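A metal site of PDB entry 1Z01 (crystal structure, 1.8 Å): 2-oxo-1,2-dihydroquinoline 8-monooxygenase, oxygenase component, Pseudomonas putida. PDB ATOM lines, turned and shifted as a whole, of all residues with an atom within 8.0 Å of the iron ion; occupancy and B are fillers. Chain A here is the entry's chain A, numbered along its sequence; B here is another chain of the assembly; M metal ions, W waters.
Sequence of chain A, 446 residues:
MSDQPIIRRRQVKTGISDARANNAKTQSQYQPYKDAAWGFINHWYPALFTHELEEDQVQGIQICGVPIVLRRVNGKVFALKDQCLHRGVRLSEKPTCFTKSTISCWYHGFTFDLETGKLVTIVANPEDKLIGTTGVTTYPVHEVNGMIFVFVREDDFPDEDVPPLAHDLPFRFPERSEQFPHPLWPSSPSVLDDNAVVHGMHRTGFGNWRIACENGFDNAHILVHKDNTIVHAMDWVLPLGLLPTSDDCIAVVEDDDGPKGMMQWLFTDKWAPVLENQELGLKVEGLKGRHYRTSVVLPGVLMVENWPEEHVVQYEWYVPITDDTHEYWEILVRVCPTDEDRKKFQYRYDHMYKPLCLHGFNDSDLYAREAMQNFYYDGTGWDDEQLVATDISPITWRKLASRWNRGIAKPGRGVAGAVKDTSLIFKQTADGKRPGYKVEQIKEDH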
ATOM      1  N   ASN A 215       2.444  19.112  25.401  1.00  0.00           N
ATOM      2  CA  ASN A 215       1.634  18.954  24.208  1.00  0.00           C
ATOM      3  C   ASN A 215       1.490  20.243  23.399  1.00  0.00           C
ATOM      4  O   ASN A 215       1.593  20.228  22.166  1.00  0.00           O
ATOM      5  CB  ASN A 215       0.253  18.413  24.615  1.00  0.00           C
ATOM      6  CG  ASN A 215      -0.789  18.584  23.525  1.00  0.00           C
ATOM      7  OD1 ASN A 215      -1.408  19.646  23.381  1.00  0.00           O
ATOM      8  ND2 ASN A 215      -0.993  17.533  22.738  1.00  0.00           N
ATOM      9  N   GLY A 216       1.270  21.348  24.090  1.00  0.00           N
ATOM     10  CA  GLY A 216       1.091  22.634  23.419  1.00  0.00           C
ATOM     11  C   GLY A 216       2.088  23.070  22.370  1.00  0.00           C
ATOM     12  O   GLY A 216       1.695  23.626  21.332  1.00  0.00           O
ATOM     13  N   PHE A 217       3.380  22.839  22.598  1.00  0.00           N
ATOM     14  CA  PHE A 217       4.394  23.273  21.636  1.00  0.00           C
ATOM     15  C   PHE A 217       5.032  22.136  20.837  1.00  0.00           C
ATOM     16  O   PHE A 217       6.141  22.268  20.308  1.00  0.00           O
ATOM     17  CB  PHE A 217       5.456  24.103  22.354  1.00  0.00           C
ATOM     18  CG  PHE A 217       6.046  23.424  23.560  1.00  0.00           C
ATOM     19  CD1 PHE A 217       7.118  22.555  23.434  1.00  0.00           C
ATOM     20  CD2 PHE A 217       5.493  23.616  24.832  1.00  0.00           C
ATOM     21  CE1 PHE A 217       7.641  21.874  24.548  1.00  0.00           C
ATOM     22  CE2 PHE A 217       6.013  22.952  25.947  1.00  0.00           C
ATOM     23  CZ  PHE A 217       7.079  22.082  25.808  1.00  0.00           C
ATOM     24  N   ASP A 218       4.329  20.999  20.744  1.00  0.00           N
ATOM     25  CA  ASP A 218       4.815  19.846  19.999  1.00  0.00           C
ATOM     26  C   ASP A 218       4.313  20.020  18.556  1.00  0.00           C
ATOM     27  O   ASP A 218       3.111  20.164  18.327  1.00  0.00           O
ATOM     28  CB  ASP A 218       4.250  18.548  20.580  1.00  0.00           C
ATOM     29  CG  ASP A 218       4.932  17.306  20.018  1.00  0.00           C
ATOM     30  OD1 ASP A 218       5.835  16.766  20.678  1.00  0.00           O
ATOM     31  OD2 ASP A 218       4.576  16.881  18.900  1.00  0.00           O
ATOM     32  N   HIS A 221       2.029  16.778  16.928  1.00  0.00           N
ATOM     33  CA  HIS A 221       0.715  16.346  17.423  1.00  0.00           C
ATOM     34  C   HIS A 221      -0.414  16.972  16.612  1.00  0.00           C
ATOM     35  O   HIS A 221      -1.581  16.822  16.965  1.00  0.00           O
ATOM     36  CB  HIS A 221       0.551  16.700  18.903  1.00  0.00           C
ATOM     37  CG  HIS A 221       0.033  18.084  19.138  1.00  0.00           C
ATOM     38  ND1 HIS A 221       0.843  19.200  19.075  1.00  0.00           N
ATOM     39  CD2 HIS A 221      -1.215  18.538  19.387  1.00  0.00           C
ATOM     40  CE1 HIS A 221       0.115  20.271  19.295  1.00  0.00           C
ATOM     41  NE2 HIS A 221      -1.144  19.904  19.490  1.00  0.00           N
ATOM     42  N   ILE A 222      -0.065  17.660  15.532  1.00  0.00           N
ATOM     43  CA  ILE A 222      -1.048  18.295  14.670  1.00  0.00           C
ATOM     44  C   ILE A 222      -2.150  17.327  14.240  1.00  0.00           C
ATOM     45  O   ILE A 222      -3.299  17.704  14.045  1.00  0.00           O
ATOM     46  CB  ILE A 222      -0.368  18.891  13.410  1.00  0.00           C
ATOM     47  CG1 ILE A 222       0.695  19.912  13.826  1.00  0.00           C
ATOM     48  CG2 ILE A 222      -1.407  19.536  12.497  1.00  0.00           C
ATOM     49  CD1 ILE A 222       1.438  20.562  12.675  1.00  0.00           C
ATOM     50  N   LEU A 223      -1.776  16.060  14.097  1.00  0.00           N
ATOM     51  CA  LEU A 223      -2.703  15.007  13.700  1.00  0.00           C
ATOM     52  C   LEU A 223      -3.950  14.955  14.581  1.00  0.00           C
ATOM     53  O   LEU A 223      -5.021  14.555  14.135  1.00  0.00           O
ATOM     54  CB  LEU A 223      -1.983  13.653  13.742  1.00  0.00           C
ATOM     55  CG  LEU A 223      -1.917  12.837  12.451  1.00  0.00           C
ATOM     56  CD1 LEU A 223      -0.588  12.082  12.373  1.00  0.00           C
ATOM     57  CD2 LEU A 223      -3.110  11.896  12.399  1.00  0.00           C
ATOM     58  N   VAL A 224      -3.795  15.371  15.834  1.00  0.00           N
ATOM     59  CA  VAL A 224      -4.885  15.375  16.816  1.00  0.00           C
ATOM     60  C   VAL A 224      -6.047  16.299  16.421  1.00  0.00           C
ATOM     61  O   VAL A 224      -7.184  16.086  16.841  1.00  0.00           O
ATOM     62  CB  VAL A 224      -4.320  15.796  18.209  1.00  0.00           C
ATOM     63  CG1 VAL A 224      -5.454  16.164  19.165  1.00  0.00           C
ATOM     64  CG2 VAL A 224      -3.492  14.650  18.782  1.00  0.00           C
ATOM     65  N   HIS A 225      -5.758  17.306  15.611  1.00  0.00           N
ATOM     66  CA  HIS A 225      -6.761  18.277  15.182  1.00  0.00           C
ATOM     67  C   HIS A 225      -7.281  18.068  13.765  1.00  0.00           C
ATOM     68  O   HIS A 225      -8.144  18.816  13.305  1.00  0.00           O
ATOM     69  CB  HIS A 225      -6.171  19.686  15.282  1.00  0.00           C
ATOM     70  CG  HIS A 225      -5.685  20.039  16.655  1.00  0.00           C
ATOM     71  ND1 HIS A 225      -6.543  20.305  17.698  1.00  0.00           N
ATOM     72  CD2 HIS A 225      -4.428  20.149  17.155  1.00  0.00           C
ATOM     73  CE1 HIS A 225      -5.835  20.568  18.787  1.00  0.00           C
ATOM     74  NE2 HIS A 225      -4.555  20.473  18.483  1.00  0.00           N
ATOM     75  N   ASN A 228     -11.004  18.479  13.597  1.00  0.00           N
ATOM     76  CA  ASN A 228     -11.687  19.590  14.261  1.00  0.00           C
ATOM     77  C   ASN A 228     -12.563  20.373  13.283  1.00  0.00           C
ATOM     78  O   ASN A 228     -12.163  20.643  12.156  1.00  0.00           O
ATOM     79  CB  ASN A 228     -10.672  20.527  14.919  1.00  0.00           C
ATOM     80  CG  ASN A 228      -9.965  19.880  16.104  1.00  0.00           C
ATOM     81  OD1 ASN A 228     -10.391  18.845  16.611  1.00  0.00           O
ATOM     82  ND2 ASN A 228      -8.889  20.506  16.546  1.00  0.00           N
ATOM     83  N   LEU A 302       2.686  28.694  27.720  1.00  0.00           N
ATOM     84  CA  LEU A 302       2.696  28.626  26.265  1.00  0.00           C
ATOM     85  C   LEU A 302       2.134  29.922  25.685  1.00  0.00           C
ATOM     86  O   LEU A 302       1.244  30.547  26.260  1.00  0.00           O
ATOM     87  CB  LEU A 302       1.826  27.460  25.781  1.00  0.00           C
ATOM     88  CG  LEU A 302       1.588  27.350  24.272  1.00  0.00           C
ATOM     89  CD1 LEU A 302       2.836  26.799  23.599  1.00  0.00           C
ATOM     90  CD2 LEU A 302       0.399  26.449  23.986  1.00  0.00           C
ATOM     91  N   TRP A 307      -2.870  33.728  16.895  1.00  0.00           N
ATOM     92  CA  TRP A 307      -3.879  32.686  17.007  1.00  0.00           C
ATOM     93  C   TRP A 307      -5.013  33.134  17.928  1.00  0.00           C
ATOM     94  O   TRP A 307      -4.775  33.690  19.006  1.00  0.00           O
ATOM     95  CB  TRP A 307      -3.232  31.411  17.543  1.00  0.00           C
ATOM     96  CG  TRP A 307      -4.144  30.233  17.590  1.00  0.00           C
ATOM     97  CD1 TRP A 307      -5.000  29.894  18.594  1.00  0.00           C
ATOM     98  CD2 TRP A 307      -4.327  29.255  16.550  1.00  0.00           C
ATOM     99  NE1 TRP A 307      -5.713  28.771  18.243  1.00  0.00           N
ATOM    100  CE2 TRP A 307      -5.314  28.363  17.002  1.00  0.00           C
ATOM    101  CE3 TRP A 307      -3.753  29.062  15.283  1.00  0.00           C
ATOM    102  CZ2 TRP A 307      -5.750  27.275  16.231  1.00  0.00           C
ATOM    103  CZ3 TRP A 307      -4.185  27.987  14.517  1.00  0.00           C
ATOM    104  CH2 TRP A 307      -5.168  27.104  14.999  1.00  0.00           C
ATOM    105  N   GLN A 314      -3.017  33.435  22.029  1.00  0.00           N
ATOM    106  CA  GLN A 314      -3.494  32.450  23.004  1.00  0.00           C
ATOM    107  C   GLN A 314      -2.406  32.076  24.000  1.00  0.00           C
ATOM    108  O   GLN A 314      -1.271  31.791  23.618  1.00  0.00           O
ATOM    109  CB  GLN A 314      -3.993  31.185  22.304  1.00  0.00           C
ATOM    110  CG  GLN A 314      -4.625  30.152  23.257  1.00  0.00           C
ATOM    111  CD  GLN A 314      -5.322  29.026  22.509  1.00  0.00           C
ATOM    112  OE1 GLN A 314      -6.059  29.264  21.540  1.00  0.00           O
ATOM    113  NE2 GLN A 314      -5.117  27.783  22.959  1.00  0.00           N
ATOM    114  N   GLU A 316      -1.530  29.654  27.525  1.00  0.00           N
ATOM    115  CA  GLU A 316      -1.966  28.517  28.327  1.00  0.00           C
ATOM    116  C   GLU A 316      -1.002  28.285  29.474  1.00  0.00           C
ATOM    117  O   GLU A 316       0.204  28.500  29.361  1.00  0.00           O
ATOM    118  CB  GLU A 316      -2.050  27.246  27.480  1.00  0.00           C
ATOM    119  CG  GLU A 316      -2.897  27.390  26.229  1.00  0.00           C
ATOM    120  CD  GLU A 316      -3.197  26.064  25.566  1.00  0.00           C
ATOM    121  OE1 GLU A 316      -2.433  25.094  25.752  1.00  0.00           O
ATOM    122  OE2 GLU A 316      -4.189  25.999  24.827  1.00  0.00           O
ATOM    123  N   PHE A 361     -11.329  22.703  19.206  1.00  0.00           N
ATOM    124  CA  PHE A 361      -9.921  22.554  18.862  1.00  0.00           C
ATOM    125  C   PHE A 361      -9.120  22.078  20.080  1.00  0.00           C
ATOM    126  O   PHE A 361      -8.533  21.007  20.058  1.00  0.00           O
ATOM    127  CB  PHE A 361      -9.342  23.897  18.375  1.00  0.00           C
ATOM    128  CG  PHE A 361      -7.973  23.775  17.749  1.00  0.00           C
ATOM    129  CD1 PHE A 361      -7.830  23.372  16.425  1.00  0.00           C
ATOM    130  CD2 PHE A 361      -6.827  24.043  18.489  1.00  0.00           C
ATOM    131  CE1 PHE A 361      -6.571  23.243  15.831  1.00  0.00           C
ATOM    132  CE2 PHE A 361      -5.555  23.922  17.904  1.00  0.00           C
ATOM    133  CZ  PHE A 361      -5.434  23.521  16.575  1.00  0.00           C
ATOM    134  N   ASN A 362      -9.127  22.879  21.143  1.00  0.00           N
ATOM    135  CA  ASN A 362      -8.369  22.542  22.352  1.00  0.00           C
ATOM    136  C   ASN A 362      -8.892  21.368  23.161  1.00  0.00           C
ATOM    137  O   ASN A 362      -8.149  20.765  23.937  1.00  0.00           O
ATOM    138  CB  ASN A 362      -8.227  23.762  23.251  1.00  0.00           C
ATOM    139  CG  ASN A 362      -7.192  24.758  22.723  1.00  0.00           C
ATOM    140  OD1 ASN A 362      -7.542  25.790  22.149  1.00  0.00           O
ATOM    141  ND2 ASN A 362      -5.916  24.431  22.922  1.00  0.00           N
ATOM    142  N   ASP A 363     -10.174  21.030  23.017  1.00  0.00           N
ATOM    143  CA  ASP A 363     -10.712  19.882  23.736  1.00  0.00           C
ATOM    144  C   ASP A 363      -9.956  18.638  23.271  1.00  0.00           C
ATOM    145  O   ASP A 363      -9.766  17.702  24.041  1.00  0.00           O
ATOM    146  CB  ASP A 363     -12.211  19.726  23.456  1.00  0.00           C
ATOM    147  CG  ASP A 363     -13.067  20.685  24.286  1.00  0.00           C
ATOM    148  OD1 ASP A 363     -14.273  20.760  24.014  1.00  0.00           O
ATOM    149  OD2 ASP A 363     -12.544  21.338  25.214  1.00  0.00           O
ATOM    150  N   SER A 364      -9.519  18.616  22.019  1.00  0.00           N
ATOM    151  CA  SER A 364      -8.760  17.488  21.485  1.00  0.00           C
ATOM    152  C   SER A 364      -7.437  17.344  22.231  1.00  0.00           C
ATOM    153  O   SER A 364      -7.003  16.228  22.528  1.00  0.00           O
ATOM    154  CB  SER A 364      -8.495  17.671  19.985  1.00  0.00           C
ATOM    155  OG  SER A 364      -9.682  17.573  19.219  1.00  0.00           O
ATOM    156  N   ASP A 365      -6.808  18.471  22.530  1.00  0.00           N
ATOM    157  CA  ASP A 365      -5.549  18.467  23.264  1.00  0.00           C
ATOM    158  C   ASP A 365      -5.771  17.985  24.691  1.00  0.00           C
ATOM    159  O   ASP A 365      -4.931  17.314  25.278  1.00  0.00           O
ATOM    160  CB  ASP A 365      -4.973  19.889  23.307  1.00  0.00           C
ATOM    161  CG  ASP A 365      -4.439  20.341  21.977  1.00  0.00           C
ATOM    162  OD1 ASP A 365      -4.583  21.529  21.665  1.00  0.00           O
ATOM    163  OD2 ASP A 365      -3.861  19.513  21.243  1.00  0.00           O
ATOM    164  N   LEU A 366      -6.923  18.339  25.252  1.00  0.00           N
ATOM    165  CA  LEU A 366      -7.268  17.983  26.618  1.00  0.00           C
ATOM    166  C   LEU A 366      -7.261  16.472  26.815  1.00  0.00           C
ATOM    167  O   LEU A 366      -6.654  15.955  27.751  1.00  0.00           O
ATOM    168  CB  LEU A 366      -8.637  18.577  26.961  1.00  0.00           C
ATOM    169  CG  LEU A 366      -9.256  18.599  28.370  1.00  0.00           C
ATOM    170  CD1 LEU A 366     -10.294  17.521  28.475  1.00  0.00           C
ATOM    171  CD2 LEU A 366      -8.187  18.447  29.429  1.00  0.00           C
ATOM    172  N   ALA A 368      -5.934  14.231  24.690  1.00  0.00           N
ATOM    173  CA  ALA A 368      -4.659  13.665  24.242  1.00  0.00           C
ATOM    174  C   ALA A 368      -3.678  13.666  25.419  1.00  0.00           C
ATOM    175  O   ALA A 368      -2.958  12.698  25.619  1.00  0.00           O
ATOM    176  CB  ALA A 368      -4.096  14.490  23.095  1.00  0.00           C
ATOM    177  N   ARG A 369      -3.682  14.752  26.183  1.00  0.00           N
ATOM    178  CA  ARG A 369      -2.808  14.890  27.353  1.00  0.00           C
ATOM    179  C   ARG A 369      -3.122  13.828  28.391  1.00  0.00           C
ATOM    180  O   ARG A 369      -2.210  13.231  28.970  1.00  0.00           O
ATOM    181  CB  ARG A 369      -3.008  16.254  28.022  1.00  0.00           C
ATOM    182  CG  ARG A 369      -2.688  17.441  27.181  1.00  0.00           C
ATOM    183  CD  ARG A 369      -3.204  18.686  27.865  1.00  0.00           C
ATOM    184  NE  ARG A 369      -3.205  19.834  26.967  1.00  0.00           N
ATOM    185  CZ  ARG A 369      -4.041  20.859  27.077  1.00  0.00           C
ATOM    186  NH1 ARG A 369      -3.962  21.857  26.200  1.00  0.00           N
ATOM    187  NH2 ARG A 369      -4.947  20.885  28.044  1.00  0.00           N
ATOM    188  N   TYR B 107      -1.993  10.136  18.082  1.00  0.00           N
ATOM    189  CA  TYR B 107      -1.343  11.285  18.679  1.00  0.00           C
ATOM    190  C   TYR B 107      -0.232  11.892  17.819  1.00  0.00           C
ATOM    191  O   TYR B 107      -0.377  13.024  17.351  1.00  0.00           O
ATOM    192  CB  TYR B 107      -0.801  10.898  20.055  1.00  0.00           C
ATOM    193  CG  TYR B 107      -0.678  12.045  21.030  1.00  0.00           C
ATOM    194  CD1 TYR B 107      -0.479  11.790  22.385  1.00  0.00           C
ATOM    195  CD2 TYR B 107      -0.751  13.378  20.621  1.00  0.00           C
ATOM    196  CE1 TYR B 107      -0.366  12.826  23.306  1.00  0.00           C
ATOM    197  CE2 TYR B 107      -0.639  14.420  21.526  1.00  0.00           C
ATOM    198  CZ  TYR B 107      -0.449  14.141  22.871  1.00  0.00           C
ATOM    199  OH  TYR B 107      -0.356  15.166  23.795  1.00  0.00           O
HETATM  200 FE    FE M   1      -3.060  20.995  19.804  1.00  0.00          FE
HETATM  201  O   HOH W   1      -2.269  23.032  19.211  1.00  0.00           O
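A ring nitrogen (ND1) of His 225 lies close to the backbone carbonyl oxygen (O) of Phe 361 (3.2 Å). A ring nitrogen (ND1) of His 225 lies within hydrogen-bond range of the side-chain amide nitrogen (ND2) of Asn 228 (2.6 Å). OD2 of Asp 365 lies close to OD1 of Asn 215 (3.3 Å). The side-chain carboxylate (OD1) of Asp 365 lies close to the side-chain amide nitrogen (ND2) of Asn 362. NE of Arg 369 lies close to O of Asp 365. A ring nitrogen (ND1) of His 221 lies close to the backbone carbonyl oxygen (O) of Asn 215, 3.3 Å away. A ring nitrogen (ND1) of His 221 lies within hydrogen-bond range of the backbone carbonyl oxygen of Asp 218 (2.6 Å).
Three residues have an atom within 4 Å of the iron ion: His 221, His 225 and Asp 365. The nearest printed residue that does not touch the iron ion is Asn 215 (4.2 Å).
The iron ion is bound by NE2 of His 225, OD2 of Asp 365, NE2 of His 221, water W1 and OD1 of Asp 365. The iron ion has five donor atoms within binding distance.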
